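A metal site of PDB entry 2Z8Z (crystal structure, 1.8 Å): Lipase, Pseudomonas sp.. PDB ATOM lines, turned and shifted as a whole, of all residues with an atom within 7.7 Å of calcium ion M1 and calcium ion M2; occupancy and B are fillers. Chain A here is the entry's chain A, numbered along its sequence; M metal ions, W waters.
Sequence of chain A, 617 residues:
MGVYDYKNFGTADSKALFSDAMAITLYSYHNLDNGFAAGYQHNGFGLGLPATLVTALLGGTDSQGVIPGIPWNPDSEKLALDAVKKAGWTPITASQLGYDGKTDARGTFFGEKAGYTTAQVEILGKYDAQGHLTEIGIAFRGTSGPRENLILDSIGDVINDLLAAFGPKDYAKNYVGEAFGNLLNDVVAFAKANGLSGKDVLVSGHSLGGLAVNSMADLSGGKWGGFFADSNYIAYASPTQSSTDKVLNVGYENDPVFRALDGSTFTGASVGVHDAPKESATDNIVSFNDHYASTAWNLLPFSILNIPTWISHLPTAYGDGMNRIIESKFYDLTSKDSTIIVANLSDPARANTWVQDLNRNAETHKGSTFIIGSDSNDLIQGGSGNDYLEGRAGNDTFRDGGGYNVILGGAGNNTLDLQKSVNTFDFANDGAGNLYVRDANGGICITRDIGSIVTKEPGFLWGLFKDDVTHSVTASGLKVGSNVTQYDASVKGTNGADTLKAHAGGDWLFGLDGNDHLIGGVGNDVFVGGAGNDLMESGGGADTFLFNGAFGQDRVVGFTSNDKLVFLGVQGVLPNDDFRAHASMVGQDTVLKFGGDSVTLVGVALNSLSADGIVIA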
ATOM      1  N   ASN A 249       5.905  24.977 -38.015  1.00  0.00           N
ATOM      2  CA  ASN A 249       4.443  24.890 -37.813  1.00  0.00           C
ATOM      3  C   ASN A 249       4.102  25.211 -36.368  1.00  0.00           C
ATOM      4  O   ASN A 249       4.294  24.389 -35.457  1.00  0.00           O
ATOM      5  CB  ASN A 249       3.924  23.497 -38.210  1.00  0.00           C
ATOM      6  CG  ASN A 249       3.744  23.346 -39.730  1.00  0.00           C
ATOM      7  OD1 ASN A 249       4.420  22.499 -40.392  1.00  0.00           O
ATOM      8  ND2 ASN A 249       2.897  24.168 -40.305  1.00  0.00           N
ATOM      9  N   GLU A 253      -1.975  23.885 -28.903  1.00  0.00           N
ATOM     10  CA  GLU A 253      -2.227  22.452 -28.716  1.00  0.00           C
ATOM     11  C   GLU A 253      -3.730  22.167 -28.774  1.00  0.00           C
ATOM     12  O   GLU A 253      -4.161  21.075 -29.251  1.00  0.00           O
ATOM     13  CB  GLU A 253      -1.691  22.060 -27.337  1.00  0.00           C
ATOM     14  CG  GLU A 253      -1.872  20.736 -26.913  1.00  0.00           C
ATOM     15  CD  GLU A 253      -1.261  20.479 -25.566  1.00  0.00           C
ATOM     16  OE1 GLU A 253      -1.867  20.823 -24.527  1.00  0.00           O
ATOM     17  OE2 GLU A 253      -0.226  19.834 -25.564  1.00  0.00           O
ATOM     18  N   ASN A 254      -4.514  23.105 -28.249  1.00  0.00           N
ATOM     19  CA  ASN A 254      -5.962  22.911 -28.109  1.00  0.00           C
ATOM     20  C   ASN A 254      -6.737  23.504 -29.283  1.00  0.00           C
ATOM     21  O   ASN A 254      -7.955  23.612 -29.264  1.00  0.00           O
ATOM     22  CB  ASN A 254      -6.486  23.381 -26.732  1.00  0.00           C
ATOM     23  CG  ASN A 254      -6.065  24.761 -26.347  1.00  0.00           C
ATOM     24  OD1 ASN A 254      -4.925  25.206 -26.569  1.00  0.00           O
ATOM     25  ND2 ASN A 254      -6.985  25.456 -25.653  1.00  0.00           N
ATOM     26  N   ARG A 259      -2.614  20.606 -36.831  1.00  0.00           N
ATOM     27  CA  ARG A 259      -2.077  19.247 -36.908  1.00  0.00           C
ATOM     28  C   ARG A 259      -3.212  18.199 -37.090  1.00  0.00           C
ATOM     29  O   ARG A 259      -3.081  16.959 -36.759  1.00  0.00           O
ATOM     30  CB  ARG A 259      -1.254  18.922 -35.663  1.00  0.00           C
ATOM     31  CG  ARG A 259      -0.087  19.878 -35.346  1.00  0.00           C
ATOM     32  CD  ARG A 259       0.466  19.585 -33.906  1.00  0.00           C
ATOM     33  NE  ARG A 259      -0.567  19.701 -32.891  1.00  0.00           N
ATOM     34  CZ  ARG A 259      -0.499  19.241 -31.633  1.00  0.00           C
ATOM     35  NH1 ARG A 259       0.583  18.594 -31.237  1.00  0.00           N
ATOM     36  NH2 ARG A 259      -1.514  19.402 -30.797  1.00  0.00           N
ATOM     37  N   HIS A 274      -5.576  15.144 -31.576  1.00  0.00           N
ATOM     38  CA  HIS A 274      -4.482  14.783 -32.468  1.00  0.00           C
ATOM     39  C   HIS A 274      -3.229  15.524 -32.047  1.00  0.00           C
ATOM     40  O   HIS A 274      -2.727  16.425 -32.733  1.00  0.00           O
ATOM     41  CB  HIS A 274      -4.847  15.055 -33.948  1.00  0.00           C
ATOM     42  CG  HIS A 274      -5.604  16.313 -34.152  1.00  0.00           C
ATOM     43  ND1 HIS A 274      -5.007  17.568 -34.098  1.00  0.00           N
ATOM     44  CD2 HIS A 274      -6.919  16.537 -34.402  1.00  0.00           C
ATOM     45  CE1 HIS A 274      -5.922  18.484 -34.334  1.00  0.00           C
ATOM     46  NE2 HIS A 274      -7.091  17.899 -34.508  1.00  0.00           N
ATOM     47  N   ASP A 275      -2.696  15.066 -30.899  1.00  0.00           N
ATOM     48  CA  ASP A 275      -1.612  15.702 -30.217  1.00  0.00           C
ATOM     49  C   ASP A 275      -0.303  14.875 -30.207  1.00  0.00           C
ATOM     50  O   ASP A 275       0.595  15.051 -29.317  1.00  0.00           O
ATOM     51  CB  ASP A 275      -2.074  16.014 -28.821  1.00  0.00           C
ATOM     52  CG  ASP A 275      -1.122  16.958 -28.076  1.00  0.00           C
ATOM     53  OD1 ASP A 275      -0.535  17.914 -28.686  1.00  0.00           O
ATOM     54  OD2 ASP A 275      -0.926  16.684 -26.860  1.00  0.00           O
ATOM     55  N   ALA A 276      -0.163  13.981 -31.199  1.00  0.00           N
ATOM     56  CA  ALA A 276       1.064  13.227 -31.321  1.00  0.00           C
ATOM     57  C   ALA A 276       2.205  14.178 -31.730  1.00  0.00           C
ATOM     58  O   ALA A 276       1.987  15.167 -32.500  1.00  0.00           O
ATOM     59  CB  ALA A 276       0.918  12.005 -32.297  1.00  0.00           C
ATOM     60  N   PRO A 277       3.391  13.960 -31.150  1.00  0.00           N
ATOM     61  CA  PRO A 277       4.484  14.824 -31.532  1.00  0.00           C
ATOM     62  C   PRO A 277       4.787  14.873 -33.025  1.00  0.00           C
ATOM     63  O   PRO A 277       4.753  13.865 -33.707  1.00  0.00           O
ATOM     64  CB  PRO A 277       5.682  14.259 -30.731  1.00  0.00           C
ATOM     65  CG  PRO A 277       5.028  13.605 -29.574  1.00  0.00           C
ATOM     66  CD  PRO A 277       3.793  13.006 -30.087  1.00  0.00           C
ATOM     67  N   LYS A 278       5.149  16.074 -33.504  1.00  0.00           N
ATOM     68  CA  LYS A 278       5.552  16.252 -34.886  1.00  0.00           C
ATOM     69  C   LYS A 278       6.787  17.079 -34.987  1.00  0.00           C
ATOM     70  O   LYS A 278       6.880  18.133 -34.345  1.00  0.00           O
ATOM     71  CB  LYS A 278       4.405  16.901 -35.650  1.00  0.00           C
ATOM     72  CG  LYS A 278       3.242  15.875 -35.944  1.00  0.00           C
ATOM     73  CD  LYS A 278       1.984  16.517 -36.584  1.00  0.00           C
ATOM     74  CE  LYS A 278       0.990  15.381 -37.125  1.00  0.00           C
ATOM     75  NZ  LYS A 278       0.561  14.517 -36.011  1.00  0.00           N
ATOM     76  N   GLU A 279       7.760  16.609 -35.761  1.00  0.00           N
ATOM     77  CA  GLU A 279       9.057  17.278 -35.843  1.00  0.00           C
ATOM     78  C   GLU A 279       9.014  18.755 -36.252  1.00  0.00           C
ATOM     79  O   GLU A 279       9.750  19.594 -35.725  1.00  0.00           O
ATOM     80  CB  GLU A 279       9.988  16.516 -36.784  1.00  0.00           C
ATOM     81  CG  GLU A 279      11.422  17.036 -36.791  1.00  0.00           C
ATOM     82  CD  GLU A 279      11.658  18.170 -37.781  1.00  0.00           C
ATOM     83  OE1 GLU A 279      10.799  18.383 -38.704  1.00  0.00           O
ATOM     84  OE2 GLU A 279      12.741  18.852 -37.653  1.00  0.00           O
ATOM     85  N   SER A 280       8.188  19.095 -37.221  1.00  0.00           N
ATOM     86  CA  SER A 280       8.069  20.460 -37.648  1.00  0.00           C
ATOM     87  C   SER A 280       7.276  21.438 -36.709  1.00  0.00           C
ATOM     88  O   SER A 280       7.315  22.670 -36.872  1.00  0.00           O
ATOM     89  CB  SER A 280       7.413  20.493 -39.027  1.00  0.00           C
ATOM     90  OG  SER A 280       6.002  20.341 -38.934  1.00  0.00           O
ATOM     91  N   ALA A 281       6.523  20.886 -35.748  1.00  0.00           N
ATOM     92  CA  ALA A 281       5.534  21.658 -34.981  1.00  0.00           C
ATOM     93  C   ALA A 281       5.907  21.934 -33.543  1.00  0.00           C
ATOM     94  O   ALA A 281       6.551  21.119 -32.893  1.00  0.00           O
ATOM     95  CB  ALA A 281       4.255  20.909 -34.989  1.00  0.00           C
ATOM     96  N   THR A 282       5.407  23.055 -33.001  1.00  0.00           N
ATOM     97  CA  THR A 282       5.412  23.319 -31.583  1.00  0.00           C
ATOM     98  C   THR A 282       4.231  22.545 -30.963  1.00  0.00           C
ATOM     99  O   THR A 282       3.106  22.837 -31.229  1.00  0.00           O
ATOM    100  CB  THR A 282       5.232  24.810 -31.294  1.00  0.00           C
ATOM    101  OG1 THR A 282       4.037  25.221 -31.925  1.00  0.00           O
ATOM    102  CG2 THR A 282       6.400  25.610 -31.873  1.00  0.00           C
ATOM    103  N   ASP A 283       4.514  21.526 -30.187  1.00  0.00           N
ATOM    104  CA  ASP A 283       3.462  20.605 -29.789  1.00  0.00           C
ATOM    105  C   ASP A 283       2.728  20.859 -28.463  1.00  0.00           C
ATOM    106  O   ASP A 283       1.731  20.179 -28.217  1.00  0.00           O
ATOM    107  CB  ASP A 283       3.969  19.167 -29.853  1.00  0.00           C
ATOM    108  CG  ASP A 283       4.230  18.699 -31.301  1.00  0.00           C
ATOM    109  OD1 ASP A 283       3.306  18.839 -32.148  1.00  0.00           O
ATOM    110  OD2 ASP A 283       5.340  18.173 -31.597  1.00  0.00           O
ATOM    111  N   ASN A 284       3.179  21.820 -27.649  1.00  0.00           N
ATOM    112  CA  ASN A 284       2.731  21.898 -26.269  1.00  0.00           C
ATOM    113  C   ASN A 284       2.479  23.325 -25.789  1.00  0.00           C
ATOM    114  O   ASN A 284       2.691  23.602 -24.643  1.00  0.00           O
ATOM    115  CB  ASN A 284       3.748  21.194 -25.330  1.00  0.00           C
ATOM    116  CG  ASN A 284       4.044  19.785 -25.752  1.00  0.00           C
ATOM    117  OD1 ASN A 284       5.199  19.403 -26.037  1.00  0.00           O
ATOM    118  ND2 ASN A 284       3.001  18.968 -25.748  1.00  0.00           N
ATOM    119  N   ILE A 285       1.966  24.154 -26.671  1.00  0.00           N
ATOM    120  CA  ILE A 285       1.584  25.525 -26.303  1.00  0.00           C
ATOM    121  C   ILE A 285       0.075  25.548 -26.111  1.00  0.00           C
ATOM    122  O   ILE A 285      -0.689  25.416 -27.081  1.00  0.00           O
ATOM    123  CB  ILE A 285       1.976  26.562 -27.385  1.00  0.00           C
ATOM    124  CG1 ILE A 285       3.489  26.504 -27.759  1.00  0.00           C
ATOM    125  CG2 ILE A 285       1.707  27.982 -26.848  1.00  0.00           C
ATOM    126  CD1 ILE A 285       3.901  27.366 -28.889  1.00  0.00           C
ATOM    127  N   VAL A 286      -0.356  25.823 -24.879  1.00  0.00           N
ATOM    128  CA  VAL A 286      -1.790  25.802 -24.533  1.00  0.00           C
ATOM    129  C   VAL A 286      -2.375  27.156 -24.566  1.00  0.00           C
ATOM    130  O   VAL A 286      -1.789  28.093 -24.009  1.00  0.00           O
ATOM    131  CB  VAL A 286      -2.017  25.214 -23.140  1.00  0.00           C
ATOM    132  CG1 VAL A 286      -3.464  25.334 -22.695  1.00  0.00           C
ATOM    133  CG2 VAL A 286      -1.578  23.823 -23.093  1.00  0.00           C
ATOM    134  N   LYS A 336      11.289  24.071 -28.796  1.00  0.00           N
ATOM    135  CA  LYS A 336      10.155  23.977 -29.717  1.00  0.00           C
ATOM    136  C   LYS A 336       8.968  23.273 -29.068  1.00  0.00           C
ATOM    137  O   LYS A 336       7.829  23.655 -29.295  1.00  0.00           O
ATOM    138  CB  LYS A 336      10.587  23.206 -30.961  1.00  0.00           C
ATOM    139  CG  LYS A 336       9.597  23.238 -32.106  1.00  0.00           C
ATOM    140  CD  LYS A 336      10.315  22.834 -33.352  1.00  0.00           C
ATOM    141  CE  LYS A 336       9.464  22.784 -34.591  1.00  0.00           C
ATOM    142  NZ  LYS A 336      10.452  22.734 -35.759  1.00  0.00           N
ATOM    143  N   ASP A 337       9.250  22.255 -28.250  1.00  0.00           N
ATOM    144  CA  ASP A 337       8.206  21.459 -27.602  1.00  0.00           C
ATOM    145  C   ASP A 337       8.081  21.673 -26.082  1.00  0.00           C
ATOM    146  O   ASP A 337       7.460  20.885 -25.376  1.00  0.00           O
ATOM    147  CB  ASP A 337       8.347  19.953 -27.967  1.00  0.00           C
ATOM    148  CG  ASP A 337       8.055  19.688 -29.411  1.00  0.00           C
ATOM    149  OD1 ASP A 337       7.103  20.320 -29.948  1.00  0.00           O
ATOM    150  OD2 ASP A 337       8.767  18.870 -30.006  1.00  0.00           O
ATOM    151  N   SER A 338       8.589  22.806 -25.597  1.00  0.00           N
ATOM    152  CA  SER A 338       8.300  23.224 -24.228  1.00  0.00           C
ATOM    153  C   SER A 338       6.815  23.365 -24.024  1.00  0.00           C
ATOM    154  O   SER A 338       6.048  23.755 -24.906  1.00  0.00           O
ATOM    155  CB  SER A 338       9.003  24.568 -23.887  1.00  0.00           C
ATOM    156  OG  SER A 338      10.416  24.485 -23.874  1.00  0.00           O
ATOM    157  N   THR A 339       6.383  22.965 -22.850  1.00  0.00           N
ATOM    158  CA  THR A 339       5.034  23.186 -22.361  1.00  0.00           C
ATOM    159  C   THR A 339       4.919  24.660 -21.928  1.00  0.00           C
ATOM    160  O   THR A 339       5.580  25.144 -20.986  1.00  0.00           O
ATOM    161  CB  THR A 339       4.721  22.362 -21.143  1.00  0.00           C
ATOM    162  OG1 THR A 339       5.101  20.988 -21.344  1.00  0.00           O
ATOM    163  CG2 THR A 339       3.213  22.496 -20.778  1.00  0.00           C
ATOM    164  N   ASN A 359      -3.632  19.988 -18.578  1.00  0.00           N
ATOM    165  CA  ASN A 359      -3.280  18.896 -19.510  1.00  0.00           C
ATOM    166  C   ASN A 359      -4.510  18.302 -20.200  1.00  0.00           C
ATOM    167  O   ASN A 359      -4.571  17.117 -20.470  1.00  0.00           O
ATOM    168  CB  ASN A 359      -2.525  17.782 -18.791  1.00  0.00           C
ATOM    169  CG  ASN A 359      -1.390  17.179 -19.649  1.00  0.00           C
ATOM    170  OD1 ASN A 359      -0.250  17.125 -19.178  1.00  0.00           O
ATOM    171  ND2 ASN A 359      -1.692  16.771 -20.904  1.00  0.00           N
ATOM    172  N   ASN A 361      -7.098  17.235 -23.005  1.00  0.00           N
ATOM    173  CA  ASN A 361      -7.140  16.975 -24.445  1.00  0.00           C
ATOM    174  C   ASN A 361      -5.765  17.035 -25.089  1.00  0.00           C
ATOM    175  O   ASN A 361      -5.547  17.703 -26.104  1.00  0.00           O
ATOM    176  CB  ASN A 361      -8.108  17.954 -25.100  1.00  0.00           C
ATOM    177  CG  ASN A 361      -9.522  17.681 -24.738  1.00  0.00           C
ATOM    178  OD1 ASN A 361      -9.941  16.509 -24.664  1.00  0.00           O
ATOM    179  ND2 ASN A 361     -10.279  18.735 -24.538  1.00  0.00           N
ATOM    180  N   ALA A 362      -4.836  16.321 -24.485  1.00  0.00           N
ATOM    181  CA  ALA A 362      -3.413  16.391 -24.849  1.00  0.00           C
ATOM    182  C   ALA A 362      -2.677  15.214 -24.260  1.00  0.00           C
ATOM    183  O   ALA A 362      -3.050  14.691 -23.179  1.00  0.00           O
ATOM    184  CB  ALA A 362      -2.801  17.749 -24.313  1.00  0.00           C
ATOM    185  N   GLU A 363      -1.596  14.806 -24.919  1.00  0.00           N
ATOM    186  CA  GLU A 363      -0.702  13.816 -24.363  1.00  0.00           C
ATOM    187  C   GLU A 363      -0.075  14.388 -23.103  1.00  0.00           C
ATOM    188  O   GLU A 363      -0.034  15.592 -22.942  1.00  0.00           O
ATOM    189  CB  GLU A 363       0.342  13.479 -25.404  1.00  0.00           C
ATOM    190  CG  GLU A 363      -0.367  12.896 -26.659  1.00  0.00           C
ATOM    191  CD  GLU A 363       0.425  12.015 -27.554  1.00  0.00           C
ATOM    192  OE1 GLU A 363       1.641  11.920 -27.381  1.00  0.00           O
ATOM    193  OE2 GLU A 363      -0.238  11.473 -28.515  1.00  0.00           O
ATOM    194  N   THR A 364       0.420  13.542 -22.218  1.00  0.00           N
ATOM    195  CA  THR A 364       1.021  13.979 -20.983  1.00  0.00           C
ATOM    196  C   THR A 364       2.212  14.884 -21.193  1.00  0.00           C
ATOM    197  O   THR A 364       3.083  14.585 -21.944  1.00  0.00           O
ATOM    198  CB  THR A 364       1.402  12.792 -20.094  1.00  0.00           C
ATOM    199  OG1 THR A 364       0.170  12.109 -19.783  1.00  0.00           O
ATOM    200  CG2 THR A 364       2.055  13.259 -18.818  1.00  0.00           C
ATOM    201  N   HIS A 365       2.183  16.025 -20.556  1.00  0.00           N
ATOM    202  CA  HIS A 365       3.227  16.980 -20.762  1.00  0.00           C
ATOM    203  C   HIS A 365       4.473  16.550 -20.055  1.00  0.00           C
ATOM    204  O   HIS A 365       4.382  16.000 -18.963  1.00  0.00           O
ATOM    205  CB  HIS A 365       2.822  18.335 -20.244  1.00  0.00           C
ATOM    206  CG  HIS A 365       1.779  19.028 -21.097  1.00  0.00           C
ATOM    207  ND1 HIS A 365       0.795  19.790 -20.530  1.00  0.00           N
ATOM    208  CD2 HIS A 365       1.537  19.002 -22.430  1.00  0.00           C
ATOM    209  CE1 HIS A 365       0.005  20.269 -21.501  1.00  0.00           C
ATOM    210  NE2 HIS A 365       0.450  19.836 -22.656  1.00  0.00           N
HETATM  211 CA    CA M   1       7.421  19.020 -32.078  1.00  0.00          CA
HETATM  212 CA    CA M   2       0.968  18.331 -26.786  1.00  0.00          CA
HETATM  213  O   HOH W   1       1.408  17.016 -24.841  1.00  0.00           O
HETATM  214  O   HOH W   2       8.180  16.713 -31.926  1.00  0.00           O
HETATM  215  O   HOH W   3       2.252  16.656 -28.067  1.00  0.00           O
HETATM  216  O   HOH W   4       9.506  19.545 -32.937  1.00  0.00           O
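Of the 27 residues printed, 4 come within 4 Å of calcium ion M1.
Along chain A the residues within 4 Å of calcium ion M1 span positions 278 to 337.
Calcium ion M1 is bound by the side-chain carboxylate (OD2) of Asp 283 (2.3 Å), water W4 (2.3 Å), the backbone carbonyl oxygen (O) of Ala 281 (2.4 Å), water W2 (2.4 Å), the side-chain carboxylate (OD2) of Asp 337 (2.5 Å), the backbone carbonyl oxygen (O) of Lys 278 (2.5 Å) and the side-chain carboxylate (OD1) of Asp 337 (2.5 Å).
Calcium ion M1 has seven donor atoms within binding distance.
The side-chain carboxylate of Asp 283 is in salt-bridge range of the guanidinium group of Arg 259 (2.9 Å).
The side-chain carboxylate (OD1) of Asp 275 lies close to the guanidinium group (NH2) of Arg 259.
OD2 of Asp 275 lies close to N of Glu 363 (2.8 Å).
OD1 of Asn 284 sits close to O of Asp 337 (2.8 Å).
N of Glu 253 lies within hydrogen-bond range of O of Ile 285.
NE2 of His 365 sits at hydrogen-bond distance from OE1 of Glu 253 (3.1 Å).
The backbone carbonyl oxygen (O) of Glu 253 is in hydrogen-bond range of the guanidinium group (NH2) of Arg 259 (3.5 Å).
Calcium ion M2 is bound by OE2 of Glu 253 (2.3 Å), ND2 of Asn 284 (2.4 Å), water W1 (2.4 Å), O of Asp 283 (2.5 Å), OD1 of Asp 275 (2.5 Å), water W3 (2.5 Å) and OD2 of Asp 275 (2.5 Å).
Within 4 Å of calcium ion M2: Glu 253, Asp 275, Asp 283 and Asn 284.
Along chain A the residues within 4 Å of calcium ion M2 span positions 253 to 284.
The nearest printed residue that does not touch calcium ion M2 is His 365 (4.4 Å).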
